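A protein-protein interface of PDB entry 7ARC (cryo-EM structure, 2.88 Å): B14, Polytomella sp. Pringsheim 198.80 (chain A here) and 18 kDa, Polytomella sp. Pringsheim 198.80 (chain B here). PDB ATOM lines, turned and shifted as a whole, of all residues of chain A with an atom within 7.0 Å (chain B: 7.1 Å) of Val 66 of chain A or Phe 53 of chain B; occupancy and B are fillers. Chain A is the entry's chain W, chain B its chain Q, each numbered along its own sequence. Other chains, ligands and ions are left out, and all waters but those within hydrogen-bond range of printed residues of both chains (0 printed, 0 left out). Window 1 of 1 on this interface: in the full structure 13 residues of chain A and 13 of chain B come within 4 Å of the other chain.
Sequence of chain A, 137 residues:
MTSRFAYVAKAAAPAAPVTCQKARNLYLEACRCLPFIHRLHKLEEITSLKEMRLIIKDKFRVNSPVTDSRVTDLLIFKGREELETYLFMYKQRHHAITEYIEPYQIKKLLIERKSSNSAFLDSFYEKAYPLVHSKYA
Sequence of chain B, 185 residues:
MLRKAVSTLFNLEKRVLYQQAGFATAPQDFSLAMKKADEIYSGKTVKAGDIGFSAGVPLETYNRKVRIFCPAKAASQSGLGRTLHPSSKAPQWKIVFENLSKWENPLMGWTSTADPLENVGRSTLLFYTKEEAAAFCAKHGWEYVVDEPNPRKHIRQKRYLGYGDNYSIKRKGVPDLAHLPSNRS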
ATOM      1  N   VAL A  62      10.670  36.164  11.919  1.00  0.00           N
ATOM      2  CA  VAL A  62      11.437  35.733  10.749  1.00  0.00           C
ATOM      3  C   VAL A  62      11.976  34.315  10.944  1.00  0.00           C
ATOM      4  O   VAL A  62      12.146  33.569   9.972  1.00  0.00           O
ATOM      5  CB  VAL A  62      12.572  36.729  10.430  1.00  0.00           C
ATOM      6  CG1 VAL A  62      13.555  36.815  11.573  1.00  0.00           C
ATOM      7  CG2 VAL A  62      13.279  36.349   9.139  1.00  0.00           C
ATOM      8  N   ASN A  63      12.231  33.910  12.191  1.00  0.00           N
ATOM      9  CA  ASN A  63      12.830  32.616  12.493  1.00  0.00           C
ATOM     10  C   ASN A  63      11.798  31.570  12.910  1.00  0.00           C
ATOM     11  O   ASN A  63      12.159  30.576  13.548  1.00  0.00           O
ATOM     12  CB  ASN A  63      13.883  32.768  13.592  1.00  0.00           C
ATOM     13  CG  ASN A  63      15.113  33.513  13.124  1.00  0.00           C
ATOM     14  OD1 ASN A  63      15.656  34.354  13.838  1.00  0.00           O
ATOM     15  ND2 ASN A  63      15.561  33.207  11.913  1.00  0.00           N
ATOM     16  N   SER A  64      10.528  31.773  12.561  1.00  0.00           N
ATOM     17  CA  SER A  64       9.481  30.833  12.959  1.00  0.00           C
ATOM     18  C   SER A  64       9.662  29.400  12.452  1.00  0.00           C
ATOM     19  O   SER A  64       9.365  28.472  13.224  1.00  0.00           O
ATOM     20  CB  SER A  64       8.111  31.384  12.538  1.00  0.00           C
ATOM     21  OG  SER A  64       7.974  31.452  11.131  1.00  0.00           O
ATOM     22  N   PRO A  65      10.098  29.136  11.211  1.00  0.00           N
ATOM     23  CA  PRO A  65      10.037  27.752  10.701  1.00  0.00           C
ATOM     24  C   PRO A  65      10.805  26.726  11.521  1.00  0.00           C
ATOM     25  O   PRO A  65      10.421  25.550  11.519  1.00  0.00           O
ATOM     26  CB  PRO A  65      10.621  27.878   9.288  1.00  0.00           C
ATOM     27  CG  PRO A  65      10.337  29.266   8.900  1.00  0.00           C
ATOM     28  CD  PRO A  65      10.541  30.060  10.150  1.00  0.00           C
ATOM     29  N   VAL A  66      11.882  27.118  12.206  1.00  0.00           N
ATOM     30  CA  VAL A  66      12.707  26.141  12.907  1.00  0.00           C
ATOM     31  C   VAL A  66      11.899  25.438  13.990  1.00  0.00           C
ATOM     32  O   VAL A  66      11.061  26.046  14.667  1.00  0.00           O
ATOM     33  CB  VAL A  66      13.943  26.842  13.498  1.00  0.00           C
ATOM     34  CG1 VAL A  66      14.564  26.019  14.616  1.00  0.00           C
ATOM     35  CG2 VAL A  66      14.961  27.114  12.415  1.00  0.00           C
ATOM     36  N   THR A  67      12.151  24.136  14.155  1.00  0.00           N
ATOM     37  CA  THR A  67      11.514  23.339  15.197  1.00  0.00           C
ATOM     38  C   THR A  67      12.484  22.558  16.071  1.00  0.00           C
ATOM     39  O   THR A  67      12.075  22.100  17.145  1.00  0.00           O
ATOM     40  CB  THR A  67      10.513  22.349  14.581  1.00  0.00           C
ATOM     41  OG1 THR A  67      11.173  21.560  13.584  1.00  0.00           O
ATOM     42  CG2 THR A  67       9.346  23.089  13.945  1.00  0.00           C
ATOM     43  N   ASP A  68      13.737  22.384  15.660  1.00  0.00           N
ATOM     44  CA  ASP A  68      14.707  21.669  16.478  1.00  0.00           C
ATOM     45  C   ASP A  68      15.046  22.467  17.730  1.00  0.00           C
ATOM     46  O   ASP A  68      15.217  23.688  17.681  1.00  0.00           O
ATOM     47  CB  ASP A  68      15.973  21.387  15.672  1.00  0.00           C
ATOM     48  CG  ASP A  68      16.975  20.546  16.435  1.00  0.00           C
ATOM     49  OD1 ASP A  68      16.595  19.460  16.921  1.00  0.00           O
ATOM     50  OD2 ASP A  68      18.144  20.970  16.548  1.00  0.00           O
ATOM     51  N   SER A  69      15.135  21.768  18.864  1.00  0.00           N
ATOM     52  CA  SER A  69      15.389  22.448  20.130  1.00  0.00           C
ATOM     53  C   SER A  69      16.771  23.087  20.159  1.00  0.00           C
ATOM     54  O   SER A  69      16.931  24.204  20.660  1.00  0.00           O
ATOM     55  CB  SER A  69      15.236  21.466  21.291  1.00  0.00           C
ATOM     56  OG  SER A  69      16.328  20.566  21.337  1.00  0.00           O
ATOM     57  N   ARG A  70      17.785  22.383  19.657  1.00  0.00           N
ATOM     58  CA  ARG A  70      19.152  22.893  19.710  1.00  0.00           C
ATOM     59  C   ARG A  70      19.333  24.124  18.827  1.00  0.00           C
ATOM     60  O   ARG A  70      19.972  25.105  19.235  1.00  0.00           O
ATOM     61  CB  ARG A  70      20.119  21.776  19.328  1.00  0.00           C
ATOM     62  CG  ARG A  70      20.177  20.692  20.389  1.00  0.00           C
ATOM     63  CD  ARG A  70      20.893  19.442  19.926  1.00  0.00           C
ATOM     64  NE  ARG A  70      20.026  18.607  19.103  1.00  0.00           N
ATOM     65  CZ  ARG A  70      20.456  17.802  18.142  1.00  0.00           C
ATOM     66  NH1 ARG A  70      21.744  17.670  17.878  1.00  0.00           N
ATOM     67  NH2 ARG A  70      19.570  17.105  17.436  1.00  0.00           N
ATOM     68  N   VAL A  71      18.795  24.087  17.608  1.00  0.00           N
ATOM     69  CA  VAL A  71      18.842  25.261  16.743  1.00  0.00           C
ATOM     70  C   VAL A  71      18.089  26.416  17.387  1.00  0.00           C
ATOM     71  O   VAL A  71      18.503  27.577  17.294  1.00  0.00           O
ATOM     72  CB  VAL A  71      18.289  24.920  15.348  1.00  0.00           C
ATOM     73  CG1 VAL A  71      18.244  26.159  14.476  1.00  0.00           C
ATOM     74  CG2 VAL A  71      19.132  23.839  14.698  1.00  0.00           C
ATOM     75  N   THR A  72      16.969  26.113  18.047  1.00  0.00           N
ATOM     76  CA  THR A  72      16.232  27.139  18.778  1.00  0.00           C
ATOM     77  C   THR A  72      17.091  27.752  19.876  1.00  0.00           C
ATOM     78  O   THR A  72      17.080  28.971  20.075  1.00  0.00           O
ATOM     79  CB  THR A  72      14.951  26.539  19.359  1.00  0.00           C
ATOM     80  OG1 THR A  72      14.062  26.185  18.292  1.00  0.00           O
ATOM     81  CG2 THR A  72      14.256  27.526  20.274  1.00  0.00           C
ATOM     82  N   ASP A  73      17.842  26.918  20.598  1.00  0.00           N
ATOM     83  CA  ASP A  73      18.730  27.414  21.644  1.00  0.00           C
ATOM     84  C   ASP A  73      19.773  28.359  21.063  1.00  0.00           C
ATOM     85  O   ASP A  73      20.043  29.430  21.622  1.00  0.00           O
ATOM     86  CB  ASP A  73      19.400  26.242  22.357  1.00  0.00           C
ATOM     87  CG  ASP A  73      18.421  25.427  23.181  1.00  0.00           C
ATOM     88  OD1 ASP A  73      17.421  26.001  23.659  1.00  0.00           O
ATOM     89  OD2 ASP A  73      18.653  24.210  23.352  1.00  0.00           O
ATOM     90  N   LEU A  75      19.578  30.090  18.275  1.00  0.00           N
ATOM     91  CA  LEU A  75      18.918  31.305  17.814  1.00  0.00           C
ATOM     92  C   LEU A  75      18.600  32.231  18.980  1.00  0.00           C
ATOM     93  O   LEU A  75      18.756  33.454  18.876  1.00  0.00           O
ATOM     94  CB  LEU A  75      17.646  30.938  17.053  1.00  0.00           C
ATOM     95  CG  LEU A  75      17.847  30.425  15.629  1.00  0.00           C
ATOM     96  CD1 LEU A  75      16.519  30.045  15.009  1.00  0.00           C
ATOM     97  CD2 LEU A  75      18.553  31.465  14.781  1.00  0.00           C
ATOM     98  N   LYS A  78      21.787  33.907  20.174  1.00  0.00           N
ATOM     99  CA  LYS A  78      22.200  34.974  19.269  1.00  0.00           C
ATOM    100  C   LYS A  78      21.304  36.204  19.412  1.00  0.00           C
ATOM    101  O   LYS A  78      21.790  37.341  19.365  1.00  0.00           O
ATOM    102  CB  LYS A  78      22.223  34.460  17.831  1.00  0.00           C
ATOM    103  CG  LYS A  78      23.337  33.450  17.589  1.00  0.00           C
ATOM    104  CD  LYS A  78      23.278  32.831  16.207  1.00  0.00           C
ATOM    105  CE  LYS A  78      23.660  33.839  15.142  1.00  0.00           C
ATOM    106  NZ  LYS A  78      23.722  33.221  13.791  1.00  0.00           N
ATOM    107  N   LYS B  47      16.446  18.532  11.414  1.00  0.00           N
ATOM    108  CA  LYS B  47      15.506  18.753  10.324  1.00  0.00           C
ATOM    109  C   LYS B  47      16.145  19.594   9.224  1.00  0.00           C
ATOM    110  O   LYS B  47      16.983  20.461   9.479  1.00  0.00           O
ATOM    111  CB  LYS B  47      14.244  19.439  10.851  1.00  0.00           C
ATOM    112  CG  LYS B  47      13.154  19.642   9.813  1.00  0.00           C
ATOM    113  CD  LYS B  47      11.921  20.278  10.428  1.00  0.00           C
ATOM    114  CE  LYS B  47      10.798  20.397   9.410  1.00  0.00           C
ATOM    115  NZ  LYS B  47      11.133  21.373   8.337  1.00  0.00           N
ATOM    116  N   ALA B  48      15.744  19.317   7.984  1.00  0.00           N
ATOM    117  CA  ALA B  48      16.331  19.982   6.829  1.00  0.00           C
ATOM    118  C   ALA B  48      16.042  21.477   6.854  1.00  0.00           C
ATOM    119  O   ALA B  48      14.891  21.899   6.987  1.00  0.00           O
ATOM    120  CB  ALA B  48      15.795  19.362   5.540  1.00  0.00           C
ATOM    121  N   GLY B  49      17.099  22.278   6.720  1.00  0.00           N
ATOM    122  CA  GLY B  49      16.991  23.718   6.692  1.00  0.00           C
ATOM    123  C   GLY B  49      17.183  24.405   8.025  1.00  0.00           C
ATOM    124  O   GLY B  49      17.356  25.630   8.051  1.00  0.00           O
ATOM    125  N   ASP B  50      17.160  23.660   9.130  1.00  0.00           N
ATOM    126  CA  ASP B  50      17.295  24.269  10.449  1.00  0.00           C
ATOM    127  C   ASP B  50      18.675  24.889  10.638  1.00  0.00           C
ATOM    128  O   ASP B  50      18.802  25.960  11.241  1.00  0.00           O
ATOM    129  CB  ASP B  50      17.009  23.237  11.534  1.00  0.00           C
ATOM    130  CG  ASP B  50      15.528  23.000  11.730  1.00  0.00           C
ATOM    131  OD1 ASP B  50      14.760  23.215  10.768  1.00  0.00           O
ATOM    132  OD2 ASP B  50      15.128  22.602  12.843  1.00  0.00           O
ATOM    133  N   ILE B  51      19.718  24.230  10.132  1.00  0.00           N
ATOM    134  CA  ILE B  51      21.074  24.750  10.277  1.00  0.00           C
ATOM    135  C   ILE B  51      21.232  26.063   9.522  1.00  0.00           C
ATOM    136  O   ILE B  51      22.011  26.935   9.933  1.00  0.00           O
ATOM    137  CB  ILE B  51      22.087  23.689   9.802  1.00  0.00           C
ATOM    138  CG1 ILE B  51      22.115  22.506  10.771  1.00  0.00           C
ATOM    139  CG2 ILE B  51      23.480  24.278   9.653  1.00  0.00           C
ATOM    140  CD1 ILE B  51      22.614  22.860  12.145  1.00  0.00           C
ATOM    141  N   GLY B  52      20.509  26.233   8.414  1.00  0.00           N
ATOM    142  CA  GLY B  52      20.613  27.470   7.657  1.00  0.00           C
ATOM    143  C   GLY B  52      20.231  28.694   8.466  1.00  0.00           C
ATOM    144  O   GLY B  52      20.808  29.770   8.292  1.00  0.00           O
ATOM    145  N   PHE B  53      19.246  28.553   9.356  1.00  0.00           N
ATOM    146  CA  PHE B  53      18.908  29.644  10.266  1.00  0.00           C
ATOM    147  C   PHE B  53      20.020  29.899  11.275  1.00  0.00           C
ATOM    148  O   PHE B  53      20.285  31.051  11.636  1.00  0.00           O
ATOM    149  CB  PHE B  53      17.592  29.344  10.978  1.00  0.00           C
ATOM    150  CG  PHE B  53      16.395  29.361  10.073  1.00  0.00           C
ATOM    151  CD1 PHE B  53      16.057  28.249   9.323  1.00  0.00           C
ATOM    152  CD2 PHE B  53      15.605  30.492   9.973  1.00  0.00           C
ATOM    153  CE1 PHE B  53      14.956  28.265   8.492  1.00  0.00           C
ATOM    154  CE2 PHE B  53      14.502  30.513   9.143  1.00  0.00           C
ATOM    155  CZ  PHE B  53      14.179  29.399   8.403  1.00  0.00           C
ATOM    156  N   SER B  54      20.677  28.837  11.748  1.00  0.00           N
ATOM    157  CA  SER B  54      21.784  29.001  12.684  1.00  0.00           C
ATOM    158  C   SER B  54      22.982  29.675  12.029  1.00  0.00           C
ATOM    159  O   SER B  54      23.775  30.326  12.715  1.00  0.00           O
ATOM    160  CB  SER B  54      22.192  27.648  13.265  1.00  0.00           C
ATOM    161  OG  SER B  54      22.731  26.805  12.264  1.00  0.00           O
ATOM    162  N   ALA B  55      23.138  29.514  10.713  1.00  0.00           N
ATOM    163  CA  ALA B  55      24.308  30.051  10.025  1.00  0.00           C
ATOM    164  C   ALA B  55      24.387  31.567  10.155  1.00  0.00           C
ATOM    165  O   ALA B  55      25.481  32.130  10.272  1.00  0.00           O
ATOM    166  CB  ALA B  55      24.288  29.641   8.553  1.00  0.00           C
ATOM    167  N   GLY B  56      23.244  32.247  10.122  1.00  0.00           N
ATOM    168  CA  GLY B  56      23.200  33.684  10.285  1.00  0.00           C
ATOM    169  C   GLY B  56      23.369  34.485   9.016  1.00  0.00           C
ATOM    170  O   GLY B  56      23.426  35.719   9.085  1.00  0.00           O
ATOM    171  N   VAL B  57      23.451  33.831   7.864  1.00  0.00           N
ATOM    172  CA  VAL B  57      23.585  34.502   6.576  1.00  0.00           C
ATOM    173  C   VAL B  57      22.208  34.997   6.145  1.00  0.00           C
ATOM    174  O   VAL B  57      21.196  34.566   6.719  1.00  0.00           O
ATOM    175  CB  VAL B  57      24.196  33.559   5.531  1.00  0.00           C
ATOM    176  CG1 VAL B  57      25.670  33.356   5.816  1.00  0.00           C
ATOM    177  CG2 VAL B  57      23.468  32.238   5.527  1.00  0.00           C
ATOM    178  N   LEU B  59      18.728  35.067   4.494  1.00  0.00           N
ATOM    179  CA  LEU B  59      17.891  33.928   4.137  1.00  0.00           C
ATOM    180  C   LEU B  59      17.653  33.831   2.637  1.00  0.00           C
ATOM    181  O   LEU B  59      17.328  32.746   2.143  1.00  0.00           O
ATOM    182  CB  LEU B  59      16.555  34.004   4.876  1.00  0.00           C
ATOM    183  CG  LEU B  59      16.604  33.705   6.375  1.00  0.00           C
ATOM    184  CD1 LEU B  59      15.207  33.455   6.908  1.00  0.00           C
ATOM    185  CD2 LEU B  59      17.510  32.524   6.668  1.00  0.00           C
ATOM    186  N   TYR B  62      19.500  31.049   0.441  1.00  0.00           N
ATOM    187  CA  TYR B  62      18.964  29.717   0.203  1.00  0.00           C
ATOM    188  C   TYR B  62      17.908  29.675  -0.893  1.00  0.00           C
ATOM    189  O   TYR B  62      17.504  28.580  -1.296  1.00  0.00           O
ATOM    190  CB  TYR B  62      18.407  29.163   1.511  1.00  0.00           C
ATOM    191  CG  TYR B  62      19.434  29.198   2.614  1.00  0.00           C
ATOM    192  CD1 TYR B  62      20.594  28.446   2.523  1.00  0.00           C
ATOM    193  CD2 TYR B  62      19.259  30.001   3.730  1.00  0.00           C
ATOM    194  CE1 TYR B  62      21.541  28.479   3.515  1.00  0.00           C
ATOM    195  CE2 TYR B  62      20.205  30.040   4.729  1.00  0.00           C
ATOM    196  CZ  TYR B  62      21.344  29.278   4.615  1.00  0.00           C
ATOM    197  OH  TYR B  62      22.294  29.307   5.608  1.00  0.00           O
ATOM    198  N   LYS B 139      20.918  19.990   4.533  1.00  0.00           N
ATOM    199  CA  LYS B 139      21.127  20.538   5.865  1.00  0.00           C
ATOM    200  C   LYS B 139      21.010  22.053   5.868  1.00  0.00           C
ATOM    201  O   LYS B 139      20.418  22.632   6.785  1.00  0.00           O
ATOM    202  CB  LYS B 139      22.496  20.102   6.378  1.00  0.00           C
ATOM    203  CG  LYS B 139      22.839  20.569   7.768  1.00  0.00           C
ATOM    204  CD  LYS B 139      24.147  19.951   8.209  1.00  0.00           C
ATOM    205  CE  LYS B 139      25.314  20.561   7.452  1.00  0.00           C
ATOM    206  NZ  LYS B 139      25.544  21.984   7.813  1.00  0.00           N
ATOM    207  N   HIS B 140      21.565  22.717   4.854  1.00  0.00           N
ATOM    208  CA  HIS B 140      21.425  24.167   4.783  1.00  0.00           C
ATOM    209  C   HIS B 140      20.106  24.625   4.176  1.00  0.00           C
ATOM    210  O   HIS B 140      19.743  25.793   4.335  1.00  0.00           O
ATOM    211  CB  HIS B 140      22.603  24.757   4.018  1.00  0.00           C
ATOM    212  CG  HIS B 140      23.857  24.801   4.828  1.00  0.00           C
ATOM    213  ND1 HIS B 140      24.279  25.935   5.486  1.00  0.00           N
ATOM    214  CD2 HIS B 140      24.765  23.840   5.113  1.00  0.00           C
ATOM    215  CE1 HIS B 140      25.399  25.671   6.134  1.00  0.00           C
ATOM    216  NE2 HIS B 140      25.718  24.408   5.919  1.00  0.00           N
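Hydrophobic or aromatic side chains of chain A that line the printed part of chain B: Pro 65, Val 66, Val 71 and Leu 75.
Of the 15 printed residues of chain B, 5 touch a printed residue of chain A.
Printed residues of chain B that touch a printed residue of chain A: Lys 47, Asp 50, Phe 53, Ser 54 and Gly 56.
Among the printed residues, 12 pairs touch across the chains.
Among the printed residues, no Asp or Glu carboxylate lies within 4 Å of a Lys or Arg side-chain nitrogen of the other chain.
Among the printed residues, merely in contact across the chains: Val 71 of chain A with Asp 50 of chain B (3.3 Å), Asn 63 of chain A with Phe 53 of chain B (3.3 Å), Val 66 of chain A with Phe 53 of chain B (3.5 Å), Thr 67 of chain A with Lys 47 of chain B (3.5 Å), Lys 78 of chain A with Gly 56 of chain B (3.6 Å), Thr 67 of chain A with Asp 50 of chain B (3.6 Å), Leu 75 of chain A with Phe 53 of chain B (3.6 Å), Pro 65 of chain A with Phe 53 of chain B (3.9 Å), Val 66 of chain A with Asp 50 of chain B (3.9 Å) and Val 62 of chain A with Phe 53 of chain B (3.9 Å).
NZ of Lys 78 of chain A is in hydrogen-bond range of O of Ser 54 of chain B, 3.1 Å away.
OD2 of Asp 50 of chain B lies within hydrogen-bond range of N of Asp 68 of chain A (3.1 Å).
The backbone carbonyl oxygen (O) of Asp 68 of chain A is in hydrogen-bond range of the side-chain hydroxyl (OG1) of Thr 72 of chain A.
The backbone carbonyl oxygen (O) of Ile 51 of chain B sits at hydrogen-bond distance from the side-chain hydroxyl (OG) of Ser 54 of chain B (2.4 Å).
The guanidinium group of Arg 70 of chain A is in salt-bridge range of the side-chain carboxylate of Asp 68 of chain A.
The side-chain carboxylate (OD2) of Asp 68 of chain A lies within hydrogen-bond range of the backbone NH (N) of Val 71 of chain A, at 3.4 Å.
Val 66 of chain A touches just these residues of chain B: Asp 50 and Phe 53.
Of chain A, only Val 62, Asn 63, Pro 65, Val 66 and Leu 75 come within 4 Å of Phe 53 of chain B.
Gly 52 of chain B touches none of the printed residues of chain A.
Printed residues of chain B within 4 Å of Leu 75 of chain A: Phe 53 (3.6 Å).
Of the printed residues of chain B, Asn 63 of chain A touches Phe 53.
Printed residues of chain A within 4 Å of Asp 50 of chain B: Val 66, Thr 67, Asp 68 and Val 71.
Of the printed residues of chain B, Val 71 of chain A touches Asp 50 (3.3 Å).
Ala 55 of chain B touches none of the printed residues of chain A.
Leu 59 of chain B touches none of the printed residues of chain A.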
